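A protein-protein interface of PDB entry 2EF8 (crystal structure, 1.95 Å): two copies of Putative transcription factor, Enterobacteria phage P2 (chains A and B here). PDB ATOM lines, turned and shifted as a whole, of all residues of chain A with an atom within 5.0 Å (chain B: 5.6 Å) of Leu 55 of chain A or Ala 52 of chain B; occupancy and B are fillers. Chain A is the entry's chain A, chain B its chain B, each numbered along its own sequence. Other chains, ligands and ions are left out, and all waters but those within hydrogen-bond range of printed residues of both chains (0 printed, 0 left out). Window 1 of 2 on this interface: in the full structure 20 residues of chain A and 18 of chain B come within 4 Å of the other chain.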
ATOM      1  N   TYR A   8      -1.314  -6.400  33.351  1.00  0.00           N
ATOM      2  CA  TYR A   8      -1.834  -7.027  32.143  1.00  0.00           C
ATOM      3  C   TYR A   8      -1.060  -6.515  30.928  1.00  0.00           C
ATOM      4  O   TYR A   8      -0.586  -7.305  30.107  1.00  0.00           O
ATOM      5  CB  TYR A   8      -3.336  -6.760  31.986  1.00  0.00           C
ATOM      6  CG  TYR A   8      -3.881  -7.195  30.642  1.00  0.00           C
ATOM      7  CD1 TYR A   8      -3.902  -6.311  29.558  1.00  0.00           C
ATOM      8  CD2 TYR A   8      -4.263  -8.525  30.420  1.00  0.00           C
ATOM      9  CE1 TYR A   8      -4.279  -6.741  28.285  1.00  0.00           C
ATOM     10  CE2 TYR A   8      -4.635  -8.969  29.145  1.00  0.00           C
ATOM     11  CZ  TYR A   8      -4.633  -8.074  28.086  1.00  0.00           C
ATOM     12  OH  TYR A   8      -4.907  -8.516  26.819  1.00  0.00           O
ATOM     13  N   LEU A  11       2.367  -8.011  30.708  1.00  0.00           N
ATOM     14  CA  LEU A  11       2.324  -9.401  30.273  1.00  0.00           C
ATOM     15  C   LEU A  11       2.171  -9.480  28.746  1.00  0.00           C
ATOM     16  O   LEU A  11       2.879 -10.236  28.068  1.00  0.00           O
ATOM     17  CB  LEU A  11       1.150 -10.109  30.964  1.00  0.00           C
ATOM     18  CG  LEU A  11       0.837 -11.534  30.493  1.00  0.00           C
ATOM     19  CD1 LEU A  11       2.066 -12.445  30.614  1.00  0.00           C
ATOM     20  CD2 LEU A  11      -0.332 -12.083  31.350  1.00  0.00           C
ATOM     21  N   LEU A  15       4.689 -11.157  25.875  1.00  0.00           N
ATOM     22  CA  LEU A  15       4.206 -12.169  24.939  1.00  0.00           C
ATOM     23  C   LEU A  15       4.430 -11.702  23.495  1.00  0.00           C
ATOM     24  O   LEU A  15       4.720 -12.500  22.611  1.00  0.00           O
ATOM     25  CB  LEU A  15       2.713 -12.439  25.201  1.00  0.00           C
ATOM     26  CG  LEU A  15       2.354 -13.022  26.577  1.00  0.00           C
ATOM     27  CD1 LEU A  15       0.853 -13.257  26.660  1.00  0.00           C
ATOM     28  CD2 LEU A  15       3.109 -14.352  26.802  1.00  0.00           C
ATOM     29  N   LEU A  50      -6.475 -10.596  25.514  1.00  0.00           N
ATOM     30  CA  LEU A  50      -5.971 -11.924  25.166  1.00  0.00           C
ATOM     31  C   LEU A  50      -6.592 -12.827  26.235  1.00  0.00           C
ATOM     32  O   LEU A  50      -6.409 -12.569  27.423  1.00  0.00           O
ATOM     33  CB  LEU A  50      -4.457 -11.972  25.324  1.00  0.00           C
ATOM     34  CG  LEU A  50      -3.831 -13.347  25.067  1.00  0.00           C
ATOM     35  CD1 LEU A  50      -3.898 -13.658  23.575  1.00  0.00           C
ATOM     36  CD2 LEU A  50      -2.382 -13.354  25.556  1.00  0.00           C
ATOM     37  N   ASP A  51      -7.323 -13.868  25.848  1.00  0.00           N
ATOM     38  CA  ASP A  51      -7.931 -14.719  26.882  1.00  0.00           C
ATOM     39  C   ASP A  51      -7.035 -15.846  27.398  1.00  0.00           C
ATOM     40  O   ASP A  51      -5.943 -16.097  26.868  1.00  0.00           O
ATOM     41  CB  ASP A  51      -9.315 -15.260  26.431  1.00  0.00           C
ATOM     42  CG  ASP A  51      -9.236 -16.377  25.376  1.00  0.00           C
ATOM     43  OD1 ASP A  51      -8.348 -17.250  25.457  1.00  0.00           O
ATOM     44  OD2 ASP A  51     -10.113 -16.412  24.476  1.00  0.00           O
ATOM     45  N   ALA A  52      -7.499 -16.517  28.452  1.00  0.00           N
ATOM     46  CA  ALA A  52      -6.751 -17.592  29.092  1.00  0.00           C
ATOM     47  C   ALA A  52      -6.354 -18.739  28.173  1.00  0.00           C
ATOM     48  O   ALA A  52      -5.280 -19.296  28.328  1.00  0.00           O
ATOM     49  CB  ALA A  52      -7.542 -18.130  30.288  1.00  0.00           C
ATOM     50  N   LEU A  53      -7.218 -19.118  27.238  1.00  0.00           N
ATOM     51  CA  LEU A  53      -6.876 -20.199  26.306  1.00  0.00           C
ATOM     52  C   LEU A  53      -5.812 -19.741  25.293  1.00  0.00           C
ATOM     53  O   LEU A  53      -4.826 -20.444  25.045  1.00  0.00           O
ATOM     54  CB  LEU A  53      -8.129 -20.682  25.560  1.00  0.00           C
ATOM     55  CG  LEU A  53      -7.855 -21.750  24.496  1.00  0.00           C
ATOM     56  CD1 LEU A  53      -7.187 -22.990  25.127  1.00  0.00           C
ATOM     57  CD2 LEU A  53      -9.160 -22.122  23.832  1.00  0.00           C
ATOM     58  N   GLU A  54      -6.019 -18.559  24.715  1.00  0.00           N
ATOM     59  CA  GLU A  54      -5.082 -17.992  23.763  1.00  0.00           C
ATOM     60  C   GLU A  54      -3.679 -17.857  24.366  1.00  0.00           C
ATOM     61  O   GLU A  54      -2.679 -18.016  23.659  1.00  0.00           O
ATOM     62  CB  GLU A  54      -5.611 -16.642  23.279  1.00  0.00           C
ATOM     63  CG  GLU A  54      -7.010 -16.798  22.678  1.00  0.00           C
ATOM     64  CD  GLU A  54      -7.657 -15.484  22.364  1.00  0.00           C
ATOM     65  OE1 GLU A  54      -7.390 -14.504  23.081  1.00  0.00           O
ATOM     66  OE2 GLU A  54      -8.443 -15.440  21.409  1.00  0.00           O
ATOM     67  N   LEU A  55      -3.599 -17.566  25.661  1.00  0.00           N
ATOM     68  CA  LEU A  55      -2.298 -17.479  26.323  1.00  0.00           C
ATOM     69  C   LEU A  55      -1.551 -18.805  26.153  1.00  0.00           C
ATOM     70  O   LEU A  55      -0.375 -18.826  25.763  1.00  0.00           O
ATOM     71  CB  LEU A  55      -2.473 -17.177  27.816  1.00  0.00           C
ATOM     72  CG  LEU A  55      -1.302 -17.534  28.747  1.00  0.00           C
ATOM     73  CD1 LEU A  55      -0.104 -16.701  28.437  1.00  0.00           C
ATOM     74  CD2 LEU A  55      -1.706 -17.295  30.158  1.00  0.00           C
ATOM     75  N   PHE A  56      -2.217 -19.921  26.444  1.00  0.00           N
ATOM     76  CA  PHE A  56      -1.543 -21.214  26.305  1.00  0.00           C
ATOM     77  C   PHE A  56      -1.204 -21.518  24.851  1.00  0.00           C
ATOM     78  O   PHE A  56      -0.137 -22.060  24.547  1.00  0.00           O
ATOM     79  CB  PHE A  56      -2.404 -22.360  26.884  1.00  0.00           C
ATOM     80  CG  PHE A  56      -2.442 -22.382  28.383  1.00  0.00           C
ATOM     81  CD1 PHE A  56      -3.536 -21.877  29.077  1.00  0.00           C
ATOM     82  CD2 PHE A  56      -1.368 -22.905  29.105  1.00  0.00           C
ATOM     83  CE1 PHE A  56      -3.570 -21.891  30.479  1.00  0.00           C
ATOM     84  CE2 PHE A  56      -1.385 -22.927  30.502  1.00  0.00           C
ATOM     85  CZ  PHE A  56      -2.497 -22.414  31.191  1.00  0.00           C
ATOM     86  N   GLU A  57      -2.119 -21.190  23.945  1.00  0.00           N
ATOM     87  CA  GLU A  57      -1.882 -21.453  22.529  1.00  0.00           C
ATOM     88  C   GLU A  57      -0.666 -20.701  21.996  1.00  0.00           C
ATOM     89  O   GLU A  57       0.122 -21.233  21.201  1.00  0.00           O
ATOM     90  CB  GLU A  57      -3.140 -21.100  21.728  1.00  0.00           C
ATOM     91  CG  GLU A  57      -4.225 -22.129  21.986  1.00  0.00           C
ATOM     92  CD  GLU A  57      -5.582 -21.709  21.514  1.00  0.00           C
ATOM     93  OE1 GLU A  57      -6.443 -22.601  21.377  1.00  0.00           O
ATOM     94  OE2 GLU A  57      -5.806 -20.511  21.297  1.00  0.00           O
ATOM     95  N   LEU A  58      -0.514 -19.460  22.441  1.00  0.00           N
ATOM     96  CA  LEU A  58       0.605 -18.627  22.037  1.00  0.00           C
ATOM     97  C   LEU A  58       1.926 -19.219  22.573  1.00  0.00           C
ATOM     98  O   LEU A  58       2.902 -19.386  21.833  1.00  0.00           O
ATOM     99  CB  LEU A  58       0.382 -17.203  22.566  1.00  0.00           C
ATOM    100  CG  LEU A  58       1.440 -16.137  22.235  1.00  0.00           C
ATOM    101  CD1 LEU A  58       0.841 -14.739  22.386  1.00  0.00           C
ATOM    102  CD2 LEU A  58       2.657 -16.337  23.163  1.00  0.00           C
ATOM    103  N   LEU A  59       1.963 -19.542  23.857  1.00  0.00           N
ATOM    104  CA  LEU A  59       3.180 -20.096  24.438  1.00  0.00           C
ATOM    105  C   LEU A  59       3.545 -21.432  23.793  1.00  0.00           C
ATOM    106  O   LEU A  59       4.728 -21.739  23.607  1.00  0.00           O
ATOM    107  CB  LEU A  59       3.018 -20.276  25.948  1.00  0.00           C
ATOM    108  CG  LEU A  59       2.842 -18.990  26.753  1.00  0.00           C
ATOM    109  CD1 LEU A  59       2.702 -19.383  28.219  1.00  0.00           C
ATOM    110  CD2 LEU A  59       4.021 -18.030  26.546  1.00  0.00           C
ATOM    111  N   THR A  77       6.995 -17.100  32.387  1.00  0.00           N
ATOM    112  CA  THR A  77       5.951 -16.137  32.056  1.00  0.00           C
ATOM    113  C   THR A  77       5.222 -15.767  33.337  1.00  0.00           C
ATOM    114  O   THR A  77       4.999 -14.595  33.632  1.00  0.00           O
ATOM    115  CB  THR A  77       4.951 -16.715  31.026  1.00  0.00           C
ATOM    116  OG1 THR A  77       5.646 -17.057  29.809  1.00  0.00           O
ATOM    117  CG2 THR A  77       3.881 -15.687  30.711  1.00  0.00           C
ATOM    118  N   LEU B  50     -12.091 -14.872  30.647  1.00  0.00           N
ATOM    119  CA  LEU B  50     -11.092 -14.848  31.707  1.00  0.00           C
ATOM    120  C   LEU B  50      -9.838 -14.456  30.935  1.00  0.00           C
ATOM    121  O   LEU B  50      -9.461 -15.140  29.972  1.00  0.00           O
ATOM    122  CB  LEU B  50     -10.904 -16.238  32.314  1.00  0.00           C
ATOM    123  CG  LEU B  50      -9.789 -16.357  33.354  1.00  0.00           C
ATOM    124  CD1 LEU B  50     -10.248 -15.709  34.666  1.00  0.00           C
ATOM    125  CD2 LEU B  50      -9.468 -17.832  33.600  1.00  0.00           C
ATOM    126  N   ASP B  51      -9.191 -13.360  31.311  1.00  0.00           N
ATOM    127  CA  ASP B  51      -8.020 -12.964  30.548  1.00  0.00           C
ATOM    128  C   ASP B  51      -6.714 -13.634  30.982  1.00  0.00           C
ATOM    129  O   ASP B  51      -6.664 -14.370  31.968  1.00  0.00           O
ATOM    130  CB  ASP B  51      -7.888 -11.429  30.466  1.00  0.00           C
ATOM    131  CG  ASP B  51      -7.406 -10.779  31.756  1.00  0.00           C
ATOM    132  OD1 ASP B  51      -6.647 -11.401  32.518  1.00  0.00           O
ATOM    133  OD2 ASP B  51      -7.760  -9.600  31.976  1.00  0.00           O
ATOM    134  N   ALA B  52      -5.681 -13.426  30.179  1.00  0.00           N
ATOM    135  CA  ALA B  52      -4.384 -14.037  30.406  1.00  0.00           C
ATOM    136  C   ALA B  52      -3.804 -13.784  31.785  1.00  0.00           C
ATOM    137  O   ALA B  52      -3.220 -14.690  32.380  1.00  0.00           O
ATOM    138  CB  ALA B  52      -3.402 -13.572  29.320  1.00  0.00           C
ATOM    139  N   LEU B  53      -3.948 -12.561  32.289  1.00  0.00           N
ATOM    140  CA  LEU B  53      -3.414 -12.229  33.614  1.00  0.00           C
ATOM    141  C   LEU B  53      -4.244 -12.888  34.718  1.00  0.00           C
ATOM    142  O   LEU B  53      -3.694 -13.418  35.685  1.00  0.00           O
ATOM    143  CB  LEU B  53      -3.392 -10.702  33.826  1.00  0.00           C
ATOM    144  CG  LEU B  53      -2.992 -10.246  35.236  1.00  0.00           C
ATOM    145  CD1 LEU B  53      -1.541 -10.652  35.491  1.00  0.00           C
ATOM    146  CD2 LEU B  53      -3.146  -8.724  35.384  1.00  0.00           C
ATOM    147  N   GLU B  54      -5.569 -12.860  34.568  1.00  0.00           N
ATOM    148  CA  GLU B  54      -6.444 -13.454  35.571  1.00  0.00           C
ATOM    149  C   GLU B  54      -6.168 -14.951  35.686  1.00  0.00           C
ATOM    150  O   GLU B  54      -6.317 -15.539  36.764  1.00  0.00           O
ATOM    151  CB  GLU B  54      -7.913 -13.175  35.214  1.00  0.00           C
ATOM    152  CG  GLU B  54      -8.205 -11.652  35.195  1.00  0.00           C
ATOM    153  CD  GLU B  54      -9.522 -11.265  34.531  1.00  0.00           C
ATOM    154  OE1 GLU B  54      -9.999 -11.999  33.642  1.00  0.00           O
ATOM    155  OE2 GLU B  54     -10.070 -10.195  34.881  1.00  0.00           O
ATOM    156  N   LEU B  55      -5.774 -15.567  34.575  1.00  0.00           N
ATOM    157  CA  LEU B  55      -5.451 -17.001  34.582  1.00  0.00           C
ATOM    158  C   LEU B  55      -4.349 -17.263  35.602  1.00  0.00           C
ATOM    159  O   LEU B  55      -4.501 -18.112  36.486  1.00  0.00           O
ATOM    160  CB  LEU B  55      -4.994 -17.448  33.189  1.00  0.00           C
ATOM    161  CG  LEU B  55      -4.478 -18.862  32.873  1.00  0.00           C
ATOM    162  CD1 LEU B  55      -3.149 -19.110  33.491  1.00  0.00           C
ATOM    163  CD2 LEU B  55      -5.469 -19.889  33.363  1.00  0.00           C
ATOM    164  N   PHE B  56      -3.235 -16.545  35.486  1.00  0.00           N
ATOM    165  CA  PHE B  56      -2.128 -16.724  36.434  1.00  0.00           C
ATOM    166  C   PHE B  56      -2.511 -16.396  37.881  1.00  0.00           C
ATOM    167  O   PHE B  56      -2.157 -17.138  38.818  1.00  0.00           O
ATOM    168  CB  PHE B  56      -0.919 -15.868  36.036  1.00  0.00           C
ATOM    169  CG  PHE B  56      -0.200 -16.367  34.828  1.00  0.00           C
ATOM    170  CD1 PHE B  56      -0.146 -15.596  33.672  1.00  0.00           C
ATOM    171  CD2 PHE B  56       0.449 -17.601  34.847  1.00  0.00           C
ATOM    172  CE1 PHE B  56       0.545 -16.027  32.545  1.00  0.00           C
ATOM    173  CE2 PHE B  56       1.152 -18.057  33.719  1.00  0.00           C
ATOM    174  CZ  PHE B  56       1.204 -17.270  32.562  1.00  0.00           C
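Of chain B, only Ala 52 and Phe 56 come within 4 Å of Leu 55 of chain A.
Of the printed residues of chain A, Ala 52 of chain B touches Leu 11 (3.9 Å), Leu 50 (3.0 Å), Asp 51 (3.9 Å), Ala 52 (3.98 Å) and Leu 55 (3.7 Å).
Printed residues of chain B within 4 Å of Ala 52 of chain A: Leu 50, Asp 51, Ala 52 and Leu 55.
Printed residues of chain B within 4 Å of Leu 11 of chain A: Ala 52 (3.9 Å) and Leu 53 (3.8 Å).
Of the printed residues of chain A, Phe 56 of chain B touches Leu 55 and Thr 77.
Glu 54 of chain A touches none of the printed residues of chain B.
Leu 58 of chain A touches none of the printed residues of chain B.
CD2 of Tyr 8 of chain A touches OD2 of Asp 51 of chain B, at 3.98 Å.
C of Ala 52 of chain B touches CD2 of Leu 11 of chain A, 3.9 Å away.
Leu 11 of chain A touches Leu 53 of chain B.
O of Leu 50 of chain A touches CA of Asp 51 of chain B, 3.5 Å away.
Asp 51 of chain A touches Ala 52 of chain B (C to N, 3.9 Å).
Ala 52 of chain A touches Asp 51 of chain B.
Ala 52 of chain B touches Ala 52 of chain A.
Ala 52 of chain A touches Leu 55 of chain B (CB to CB, 3.9 Å).
Leu 55 of chain A touches Ala 52 of chain B (CD2 to O, 3.7 Å).
Leu 55 of chain A touches Phe 56 of chain B (CD2 to CE1, 3.5 Å).
The side-chain hydroxyl of Tyr 8 of chain A sits at hydrogen-bond distance from the backbone NH of Leu 50 of chain A.
The side-chain carboxylate (OD1) of Asp 51 of chain A lies within hydrogen-bond range of the backbone NH (N) of Leu 53 of chain A (2.8 Å).
OD1 of Asp 51 of chain A is in hydrogen-bond range of N of Glu 54 of chain A (2.8 Å).
The backbone NH (N) of Leu 53 of chain B sits at hydrogen-bond distance from the side-chain carboxylate (OD1) of Asp 51 of chain B (2.9 Å).
The backbone NH of Glu 54 of chain B is in hydrogen-bond range of the side-chain carboxylate of Asp 51 of chain B.
The backbone NH of Ala 52 of chain B sits at hydrogen-bond distance from the backbone carbonyl oxygen of Leu 50 of chain A, at 3.0 Å.
The backbone NH (N) of Ala 52 of chain A lies within hydrogen-bond range of the backbone carbonyl oxygen (O) of Leu 50 of chain B (2.8 Å).
Hydrophobic or aromatic side chains of chain A within 4 Å of the printed part of chain B: Tyr 8, Leu 11, Leu 50, Ala 52, Leu 55 and Phe 56.
Of the 7 printed residues of chain B, 6 touch a printed residue of chain A.
Hydrophobic or aromatic side chains of chain B within 4 Å of the printed part of chain A: Leu 50, Ala 52, Leu 53, Leu 55 and Phe 56.
Among the printed residues, 16 pairs touch across the chains.
Among the printed residues, no Asp or Glu carboxylate lies within 4 Å of a Lys or Arg side-chain nitrogen of the other chain.
Leu 50 of chain A touches Asp 51 of chain B, and with the chains exchanged Asp 51 of chain A touches Leu 50 of chain B.
Asp 51 of chain A touches Ala 52 of chain B, and with the chains exchanged Ala 52 of chain A touches Asp 51 of chain B.
Ala 52 of chain B touches its own counterpart, Ala 52 of chain A.
Ala 52 of chain A touches Leu 55 of chain B, and with the chains exchanged Leu 55 of chain A touches Ala 52 of chain B.
7 positions are printed for both chains.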
